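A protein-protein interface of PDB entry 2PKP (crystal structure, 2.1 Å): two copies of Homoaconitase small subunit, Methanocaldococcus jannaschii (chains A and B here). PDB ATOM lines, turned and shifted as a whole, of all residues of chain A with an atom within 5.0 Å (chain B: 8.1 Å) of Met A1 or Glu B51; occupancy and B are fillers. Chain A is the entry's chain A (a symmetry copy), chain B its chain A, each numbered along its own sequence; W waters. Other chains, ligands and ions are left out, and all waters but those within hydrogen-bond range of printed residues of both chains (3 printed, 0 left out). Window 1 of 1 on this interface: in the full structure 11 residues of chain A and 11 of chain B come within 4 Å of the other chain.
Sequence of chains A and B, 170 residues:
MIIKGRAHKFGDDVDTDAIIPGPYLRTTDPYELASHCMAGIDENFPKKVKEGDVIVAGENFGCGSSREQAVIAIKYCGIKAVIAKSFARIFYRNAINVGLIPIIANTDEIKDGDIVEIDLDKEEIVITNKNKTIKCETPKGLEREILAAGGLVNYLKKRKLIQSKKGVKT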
ATOM      1  N   MET A   1      24.778 -18.068  26.206  1.00  0.00           N
ATOM      2  CA  MET A   1      24.479 -16.888  25.358  1.00  0.00           C
ATOM      3  C   MET A   1      24.041 -17.317  23.965  1.00  0.00           C
ATOM      4  O   MET A   1      24.241 -18.461  23.550  1.00  0.00           O
ATOM      5  CB  MET A   1      25.701 -15.967  25.250  1.00  0.00           C
ATOM      6  CG  MET A   1      26.746 -16.407  24.247  1.00  0.00           C
ATOM      7  SD  MET A   1      28.161 -15.275  24.163  1.00  0.00           S
ATOM      8  CE  MET A   1      27.767 -14.299  22.711  1.00  0.00           C
ATOM      9  N   ILE A   2      23.454 -16.376  23.244  1.00  0.00           N
ATOM     10  CA  ILE A   2      22.965 -16.640  21.904  1.00  0.00           C
ATOM     11  C   ILE A   2      23.593 -15.715  20.878  1.00  0.00           C
ATOM     12  O   ILE A   2      23.635 -14.502  21.067  1.00  0.00           O
ATOM     13  CB  ILE A   2      21.432 -16.476  21.859  1.00  0.00           C
ATOM     14  CG1 ILE A   2      20.777 -17.613  22.650  1.00  0.00           C
ATOM     15  CG2 ILE A   2      20.944 -16.423  20.418  1.00  0.00           C
ATOM     16  CD1 ILE A   2      19.279 -17.436  22.850  1.00  0.00           C
ATOM     17  N   ILE A   3      24.085 -16.304  19.794  1.00  0.00           N
ATOM     18  CA  ILE A   3      24.683 -15.542  18.707  1.00  0.00           C
ATOM     19  C   ILE A   3      23.736 -15.705  17.532  1.00  0.00           C
ATOM     20  O   ILE A   3      23.493 -16.830  17.088  1.00  0.00           O
ATOM     21  CB  ILE A   3      26.070 -16.101  18.322  1.00  0.00           C
ATOM     22  CG1 ILE A   3      27.054 -15.881  19.475  1.00  0.00           C
ATOM     23  CG2 ILE A   3      26.572 -15.423  17.046  1.00  0.00           C
ATOM     24  CD1 ILE A   3      28.370 -16.606  19.297  1.00  0.00           C
ATOM     25  N   LYS A  80      31.644 -13.459  15.728  1.00  0.00           N
ATOM     26  CA  LYS A  80      31.908 -14.115  17.003  1.00  0.00           C
ATOM     27  C   LYS A  80      32.050 -15.631  16.918  1.00  0.00           C
ATOM     28  O   LYS A  80      32.620 -16.251  17.812  1.00  0.00           O
ATOM     29  CB  LYS A  80      30.796 -13.768  18.001  1.00  0.00           C
ATOM     30  CG  LYS A  80      30.954 -14.400  19.379  1.00  0.00           C
ATOM     31  CD  LYS A  80      32.192 -13.889  20.096  1.00  0.00           C
ATOM     32  CE  LYS A  80      32.262 -14.420  21.521  1.00  0.00           C
ATOM     33  NZ  LYS A  80      33.426 -13.857  22.262  1.00  0.00           N
ATOM     34  N   ILE A 118      22.662 -19.396  17.175  1.00  0.00           N
ATOM     35  CA  ILE A 118      23.468 -20.362  17.904  1.00  0.00           C
ATOM     36  C   ILE A 118      23.259 -20.200  19.405  1.00  0.00           C
ATOM     37  O   ILE A 118      23.593 -19.156  19.971  1.00  0.00           O
ATOM     38  CB  ILE A 118      24.967 -20.164  17.612  1.00  0.00           C
ATOM     39  CG1 ILE A 118      25.219 -20.233  16.103  1.00  0.00           C
ATOM     40  CG2 ILE A 118      25.787 -21.224  18.346  1.00  0.00           C
ATOM     41  CD1 ILE A 118      26.617 -19.778  15.704  1.00  0.00           C
ATOM     42  N   ASP A 119      22.699 -21.224  20.046  1.00  0.00           N
ATOM     43  CA  ASP A 119      22.475 -21.181  21.487  1.00  0.00           C
ATOM     44  C   ASP A 119      23.581 -22.023  22.103  1.00  0.00           C
ATOM     45  O   ASP A 119      23.531 -23.251  22.058  1.00  0.00           O
ATOM     46  CB  ASP A 119      21.110 -21.771  21.847  1.00  0.00           C
ATOM     47  CG  ASP A 119      20.750 -21.566  23.312  1.00  0.00           C
ATOM     48  OD1 ASP A 119      21.616 -21.773  24.183  1.00  0.00           O
ATOM     49  OD2 ASP A 119      19.593 -21.205  23.593  1.00  0.00           O
ATOM     50  N   LEU A 120      24.581 -21.355  22.668  1.00  0.00           N
ATOM     51  CA  LEU A 120      25.727 -22.043  23.259  1.00  0.00           C
ATOM     52  C   LEU A 120      25.387 -22.884  24.485  1.00  0.00           C
ATOM     53  O   LEU A 120      26.071 -23.860  24.778  1.00  0.00           O
ATOM     54  CB  LEU A 120      26.825 -21.028  23.603  1.00  0.00           C
ATOM     55  CG  LEU A 120      27.306 -20.188  22.417  1.00  0.00           C
ATOM     56  CD1 LEU A 120      28.359 -19.185  22.874  1.00  0.00           C
ATOM     57  CD2 LEU A 120      27.871 -21.096  21.348  1.00  0.00           C
ATOM     58  N   ASP A 121      24.329 -22.518  25.198  1.00  0.00           N
ATOM     59  CA  ASP A 121      23.950 -23.287  26.376  1.00  0.00           C
ATOM     60  C   ASP A 121      23.212 -24.569  26.009  1.00  0.00           C
ATOM     61  O   ASP A 121      23.412 -25.602  26.640  1.00  0.00           O
ATOM     62  CB  ASP A 121      23.095 -22.439  27.324  1.00  0.00           C
ATOM     63  CG  ASP A 121      23.907 -21.357  28.023  1.00  0.00           C
ATOM     64  OD1 ASP A 121      25.062 -21.635  28.400  1.00  0.00           O
ATOM     65  OD2 ASP A 121      23.395 -20.234  28.208  1.00  0.00           O
ATOM     66  N   ALA A 148      35.303 -18.071  27.304  1.00  0.00           N
ATOM     67  CA  ALA A 148      34.449 -17.308  28.204  1.00  0.00           C
ATOM     68  C   ALA A 148      35.132 -16.007  28.627  1.00  0.00           C
ATOM     69  O   ALA A 148      34.480 -14.976  28.791  1.00  0.00           O
ATOM     70  CB  ALA A 148      34.104 -18.145  29.433  1.00  0.00           C
ATOM     71  N   LYS B   4      20.562 -10.489  20.800  1.00  0.00           N
ATOM     72  CA  LYS B   4      19.609 -11.300  21.548  1.00  0.00           C
ATOM     73  C   LYS B   4      20.205 -11.825  22.844  1.00  0.00           C
ATOM     74  O   LYS B   4      21.277 -12.438  22.849  1.00  0.00           O
ATOM     75  CB  LYS B   4      19.120 -12.469  20.686  1.00  0.00           C
ATOM     76  CG  LYS B   4      18.131 -13.399  21.371  1.00  0.00           C
ATOM     77  CD  LYS B   4      17.433 -14.278  20.342  1.00  0.00           C
ATOM     78  CE  LYS B   4      16.441 -15.232  20.984  1.00  0.00           C
ATOM     79  NZ  LYS B   4      15.640 -15.931  19.935  1.00  0.00           N
ATOM     80  N   GLY B   5      19.500 -11.579  23.946  1.00  0.00           N
ATOM     81  CA  GLY B   5      19.973 -12.041  25.239  1.00  0.00           C
ATOM     82  C   GLY B   5      18.942 -11.855  26.334  1.00  0.00           C
ATOM     83  O   GLY B   5      17.802 -11.472  26.067  1.00  0.00           O
ATOM     84  N   ARG B   6      19.343 -12.123  27.571  1.00  0.00           N
ATOM     85  CA  ARG B   6      18.440 -11.982  28.697  1.00  0.00           C
ATOM     86  C   ARG B   6      18.394 -10.531  29.172  1.00  0.00           C
ATOM     87  O   ARG B   6      19.421  -9.856  29.255  1.00  0.00           O
ATOM     88  CB  ARG B   6      18.867 -12.903  29.849  1.00  0.00           C
ATOM     89  CG  ARG B   6      17.873 -12.931  31.009  1.00  0.00           C
ATOM     90  CD  ARG B   6      18.309 -13.892  32.115  1.00  0.00           C
ATOM     91  NE  ARG B   6      18.370 -15.277  31.649  1.00  0.00           N
ATOM     92  CZ  ARG B   6      17.327 -15.960  31.180  1.00  0.00           C
ATOM     93  NH1 ARG B   6      16.129 -15.392  31.116  1.00  0.00           N
ATOM     94  NH2 ARG B   6      17.485 -17.211  30.765  1.00  0.00           N
ATOM     95  N   HIS B   8      17.834  -7.547  31.906  1.00  0.00           N
ATOM     96  CA  HIS B   8      17.983  -7.301  33.338  1.00  0.00           C
ATOM     97  C   HIS B   8      17.303  -5.957  33.518  1.00  0.00           C
ATOM     98  O   HIS B   8      17.824  -4.924  33.097  1.00  0.00           O
ATOM     99  CB  HIS B   8      19.457  -7.243  33.737  1.00  0.00           C
ATOM    100  CG  HIS B   8      20.174  -8.548  33.560  1.00  0.00           C
ATOM    101  ND1 HIS B   8      20.787  -8.909  32.378  1.00  0.00           N
ATOM    102  CD2 HIS B   8      20.332  -9.595  34.402  1.00  0.00           C
ATOM    103  CE1 HIS B   8      21.293 -10.122  32.502  1.00  0.00           C
ATOM    104  NE2 HIS B   8      21.031 -10.563  33.718  1.00  0.00           N
ATOM    105  N   LYS B  48      25.235 -12.332  37.851  1.00  0.00           N
ATOM    106  CA  LYS B  48      24.126 -12.858  37.051  1.00  0.00           C
ATOM    107  C   LYS B  48      24.281 -12.585  35.555  1.00  0.00           C
ATOM    108  O   LYS B  48      23.896 -13.408  34.723  1.00  0.00           O
ATOM    109  CB  LYS B  48      22.794 -12.240  37.491  1.00  0.00           C
ATOM    110  CG  LYS B  48      22.382 -12.471  38.930  1.00  0.00           C
ATOM    111  CD  LYS B  48      21.141 -11.640  39.247  1.00  0.00           C
ATOM    112  CE  LYS B  48      20.652 -11.853  40.675  1.00  0.00           C
ATOM    113  NZ  LYS B  48      19.527 -10.933  41.023  1.00  0.00           N
ATOM    114  N   VAL B  49      24.829 -11.420  35.220  1.00  0.00           N
ATOM    115  CA  VAL B  49      24.988 -11.019  33.828  1.00  0.00           C
ATOM    116  C   VAL B  49      25.885 -11.934  32.997  1.00  0.00           C
ATOM    117  O   VAL B  49      26.881 -12.467  33.485  1.00  0.00           O
ATOM    118  CB  VAL B  49      25.528  -9.571  33.729  1.00  0.00           C
ATOM    119  CG1 VAL B  49      26.943  -9.499  34.282  1.00  0.00           C
ATOM    120  CG2 VAL B  49      25.492  -9.099  32.287  1.00  0.00           C
ATOM    121  N   LYS B  50      25.511 -12.110  31.734  1.00  0.00           N
ATOM    122  CA  LYS B  50      26.278 -12.935  30.808  1.00  0.00           C
ATOM    123  C   LYS B  50      26.539 -12.144  29.538  1.00  0.00           C
ATOM    124  O   LYS B  50      25.719 -11.315  29.132  1.00  0.00           O
ATOM    125  CB  LYS B  50      25.509 -14.209  30.445  1.00  0.00           C
ATOM    126  CG  LYS B  50      25.164 -15.107  31.620  1.00  0.00           C
ATOM    127  CD  LYS B  50      26.408 -15.633  32.320  1.00  0.00           C
ATOM    128  CE  LYS B  50      26.025 -16.519  33.500  1.00  0.00           C
ATOM    129  NZ  LYS B  50      27.220 -16.993  34.248  1.00  0.00           N
ATOM    130  N   GLU B  51      27.684 -12.394  28.915  1.00  0.00           N
ATOM    131  CA  GLU B  51      28.029 -11.714  27.672  1.00  0.00           C
ATOM    132  C   GLU B  51      26.849 -11.884  26.720  1.00  0.00           C
ATOM    133  O   GLU B  51      26.339 -12.992  26.549  1.00  0.00           O
ATOM    134  CB  GLU B  51      29.278 -12.344  27.057  1.00  0.00           C
ATOM    135  CG  GLU B  51      29.797 -11.621  25.828  1.00  0.00           C
ATOM    136  CD  GLU B  51      30.913 -12.383  25.127  1.00  0.00           C
ATOM    137  OE1 GLU B  51      31.537 -13.259  25.767  1.00  0.00           O
ATOM    138  OE2 GLU B  51      31.170 -12.100  23.939  1.00  0.00           O
ATOM    139  N   GLY B  52      26.402 -10.788  26.119  1.00  0.00           N
ATOM    140  CA  GLY B  52      25.282 -10.867  25.200  1.00  0.00           C
ATOM    141  C   GLY B  52      23.970 -10.412  25.811  1.00  0.00           C
ATOM    142  O   GLY B  52      22.987 -10.213  25.102  1.00  0.00           O
ATOM    143  N   ASP B  53      23.947 -10.256  27.130  1.00  0.00           N
ATOM    144  CA  ASP B  53      22.738  -9.812  27.810  1.00  0.00           C
ATOM    145  C   ASP B  53      22.462  -8.335  27.552  1.00  0.00           C
ATOM    146  O   ASP B  53      23.276  -7.626  26.958  1.00  0.00           O
ATOM    147  CB  ASP B  53      22.836 -10.068  29.314  1.00  0.00           C
ATOM    148  CG  ASP B  53      22.599 -11.519  29.669  1.00  0.00           C
ATOM    149  OD1 ASP B  53      22.209 -12.297  28.771  1.00  0.00           O
ATOM    150  OD2 ASP B  53      22.785 -11.877  30.849  1.00  0.00           O
ATOM    151  N   VAL B  54      21.304  -7.881  28.014  1.00  0.00           N
ATOM    152  CA  VAL B  54      20.880  -6.508  27.803  1.00  0.00           C
ATOM    153  C   VAL B  54      20.317  -5.885  29.075  1.00  0.00           C
ATOM    154  O   VAL B  54      19.567  -6.524  29.811  1.00  0.00           O
ATOM    155  CB  VAL B  54      19.789  -6.459  26.691  1.00  0.00           C
ATOM    156  CG1 VAL B  54      19.314  -5.038  26.462  1.00  0.00           C
ATOM    157  CG2 VAL B  54      20.344  -7.059  25.402  1.00  0.00           C
ATOM    158  N   LYS B  75      29.756  -1.939  29.031  1.00  0.00           N
ATOM    159  CA  LYS B  75      30.373  -2.538  27.853  1.00  0.00           C
ATOM    160  C   LYS B  75      31.282  -3.719  28.191  1.00  0.00           C
ATOM    161  O   LYS B  75      31.278  -4.733  27.485  1.00  0.00           O
ATOM    162  CB  LYS B  75      31.164  -1.478  27.080  1.00  0.00           C
ATOM    163  CG  LYS B  75      31.878  -1.991  25.832  1.00  0.00           C
ATOM    164  CD  LYS B  75      32.711  -0.868  25.200  1.00  0.00           C
ATOM    165  CE  LYS B  75      33.417  -1.298  23.913  1.00  0.00           C
ATOM    166  NZ  LYS B  75      34.459  -2.339  24.138  1.00  0.00           N
ATOM    167  N   TYR B  76      32.048  -3.609  29.272  1.00  0.00           N
ATOM    168  CA  TYR B  76      32.942  -4.702  29.625  1.00  0.00           C
ATOM    169  C   TYR B  76      32.311  -5.889  30.349  1.00  0.00           C
ATOM    170  O   TYR B  76      33.016  -6.792  30.805  1.00  0.00           O
ATOM    171  CB  TYR B  76      34.164  -4.170  30.380  1.00  0.00           C
ATOM    172  CG  TYR B  76      35.189  -3.606  29.422  1.00  0.00           C
ATOM    173  CD1 TYR B  76      34.975  -2.382  28.785  1.00  0.00           C
ATOM    174  CD2 TYR B  76      36.330  -4.334  29.084  1.00  0.00           C
ATOM    175  CE1 TYR B  76      35.866  -1.902  27.834  1.00  0.00           C
ATOM    176  CE2 TYR B  76      37.229  -3.864  28.131  1.00  0.00           C
ATOM    177  CZ  TYR B  76      36.989  -2.647  27.510  1.00  0.00           C
ATOM    178  OH  TYR B  76      37.858  -2.179  26.554  1.00  0.00           O
ATOM    179  N   CYS B  77      30.984  -5.886  30.439  1.00  0.00           N
ATOM    180  CA  CYS B  77      30.247  -7.001  31.032  1.00  0.00           C
ATOM    181  C   CYS B  77      29.788  -7.834  29.845  1.00  0.00           C
ATOM    182  O   CYS B  77      29.169  -8.886  30.004  1.00  0.00           O
ATOM    183  CB  CYS B  77      29.011  -6.519  31.799  1.00  0.00           C
ATOM    184  SG  CYS B  77      29.300  -6.082  33.515  1.00  0.00           S
ATOM    185  N   GLY B  78      30.097  -7.350  28.647  1.00  0.00           N
ATOM    186  CA  GLY B  78      29.692  -8.052  27.445  1.00  0.00           C
ATOM    187  C   GLY B  78      28.315  -7.598  26.995  1.00  0.00           C
ATOM    188  O   GLY B  78      27.663  -8.272  26.202  1.00  0.00           O
ATOM    189  N   ILE B  79      27.870  -6.453  27.511  1.00  0.00           N
ATOM    190  CA  ILE B  79      26.569  -5.893  27.156  1.00  0.00           C
ATOM    191  C   ILE B  79      26.729  -4.925  25.987  1.00  0.00           C
ATOM    192  O   ILE B  79      27.432  -3.922  26.088  1.00  0.00           O
ATOM    193  CB  ILE B  79      25.951  -5.170  28.365  1.00  0.00           C
ATOM    194  CG1 ILE B  79      25.664  -6.194  29.466  1.00  0.00           C
ATOM    195  CG2 ILE B  79      24.679  -4.427  27.952  1.00  0.00           C
ATOM    196  CD1 ILE B  79      25.195  -5.590  30.772  1.00  0.00           C
ATOM    197  N   LYS B  80      26.069  -5.236  24.877  1.00  0.00           N
ATOM    198  CA  LYS B  80      26.150  -4.421  23.670  1.00  0.00           C
ATOM    199  C   LYS B  80      25.097  -3.323  23.576  1.00  0.00           C
ATOM    200  O   LYS B  80      25.269  -2.362  22.828  1.00  0.00           O
ATOM    201  CB  LYS B  80      26.053  -5.322  22.433  1.00  0.00           C
ATOM    202  CG  LYS B  80      26.121  -4.586  21.100  1.00  0.00           C
ATOM    203  CD  LYS B  80      27.468  -3.913  20.894  1.00  0.00           C
ATOM    204  CE  LYS B  80      27.572  -3.304  19.504  1.00  0.00           C
ATOM    205  NZ  LYS B  80      28.920  -2.716  19.260  1.00  0.00           N
HETATM  206  O   HOH W   1      31.647 -14.497  28.143  1.00  0.00           O
HETATM  207  O   HOH W   2      23.001 -11.995  20.395  1.00  0.00           O
HETATM  208  O   HOH W   3      22.678 -14.069  24.500  1.00  0.00           O
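The side-chain carboxylate of Glu B51 lies within salt-bridge range of the side-chain amino group of Lys A80, 3.3 Å away. The side-chain sulfur (SD) of Met A1 sits close to the backbone carbonyl oxygen (O) of Glu B51 (3.8 Å).
The backbone carbonyl oxygen (O) of Met A1 sits at hydrogen-bond distance from the backbone NH (N) of Leu A120, 3.0 Å away. The side-chain carboxylate (OD2) of Asp A121 sits at hydrogen-bond distance from the backbone NH (N) of Met A1 (3.3 Å).
Among the printed residues, pairs that only touch across the chains: Ile A2 with Lys B4 (3.6 Å).
Of chain B, only Glu B51 comes within 4 Å of Met A1. Printed residues of chain B within 4 Å of Ile A2: Lys B4 (3.6 Å). Of the printed residues of chain A, Lys B4 touches Ile A2 (3.6 Å).
Of the 9 printed residues of chain A, 3 touch a printed residue of chain B. Printed residues of chain A that touch a printed residue of chain B: Met A1, Ile A2 and Lys A80. Hydrophobic or aromatic side chains of chain A that line the printed part of chain B: Met A1. Along chain A the printed residues that touch a printed residue of chain B span positions 1 to 80.
Position printed for both chains: 80. Of the 3 pairs that touch across the chains among the printed residues, none has its exchanged pair printed and touching as well.
Water W2 bridges the backbone carbonyl oxygen (O) of Ile A2 (2.7 Å) and the backbone NH (N) of Lys B4 (2.9 Å). Water W1 lies within hydrogen-bond range of OE1 of Glu B51 and O of Ala A148. Water W3 lies within hydrogen-bond range of the backbone carbonyl oxygen of Lys B4 (2.7 Å) and the backbone NH of Ile A2 (2.7 Å).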
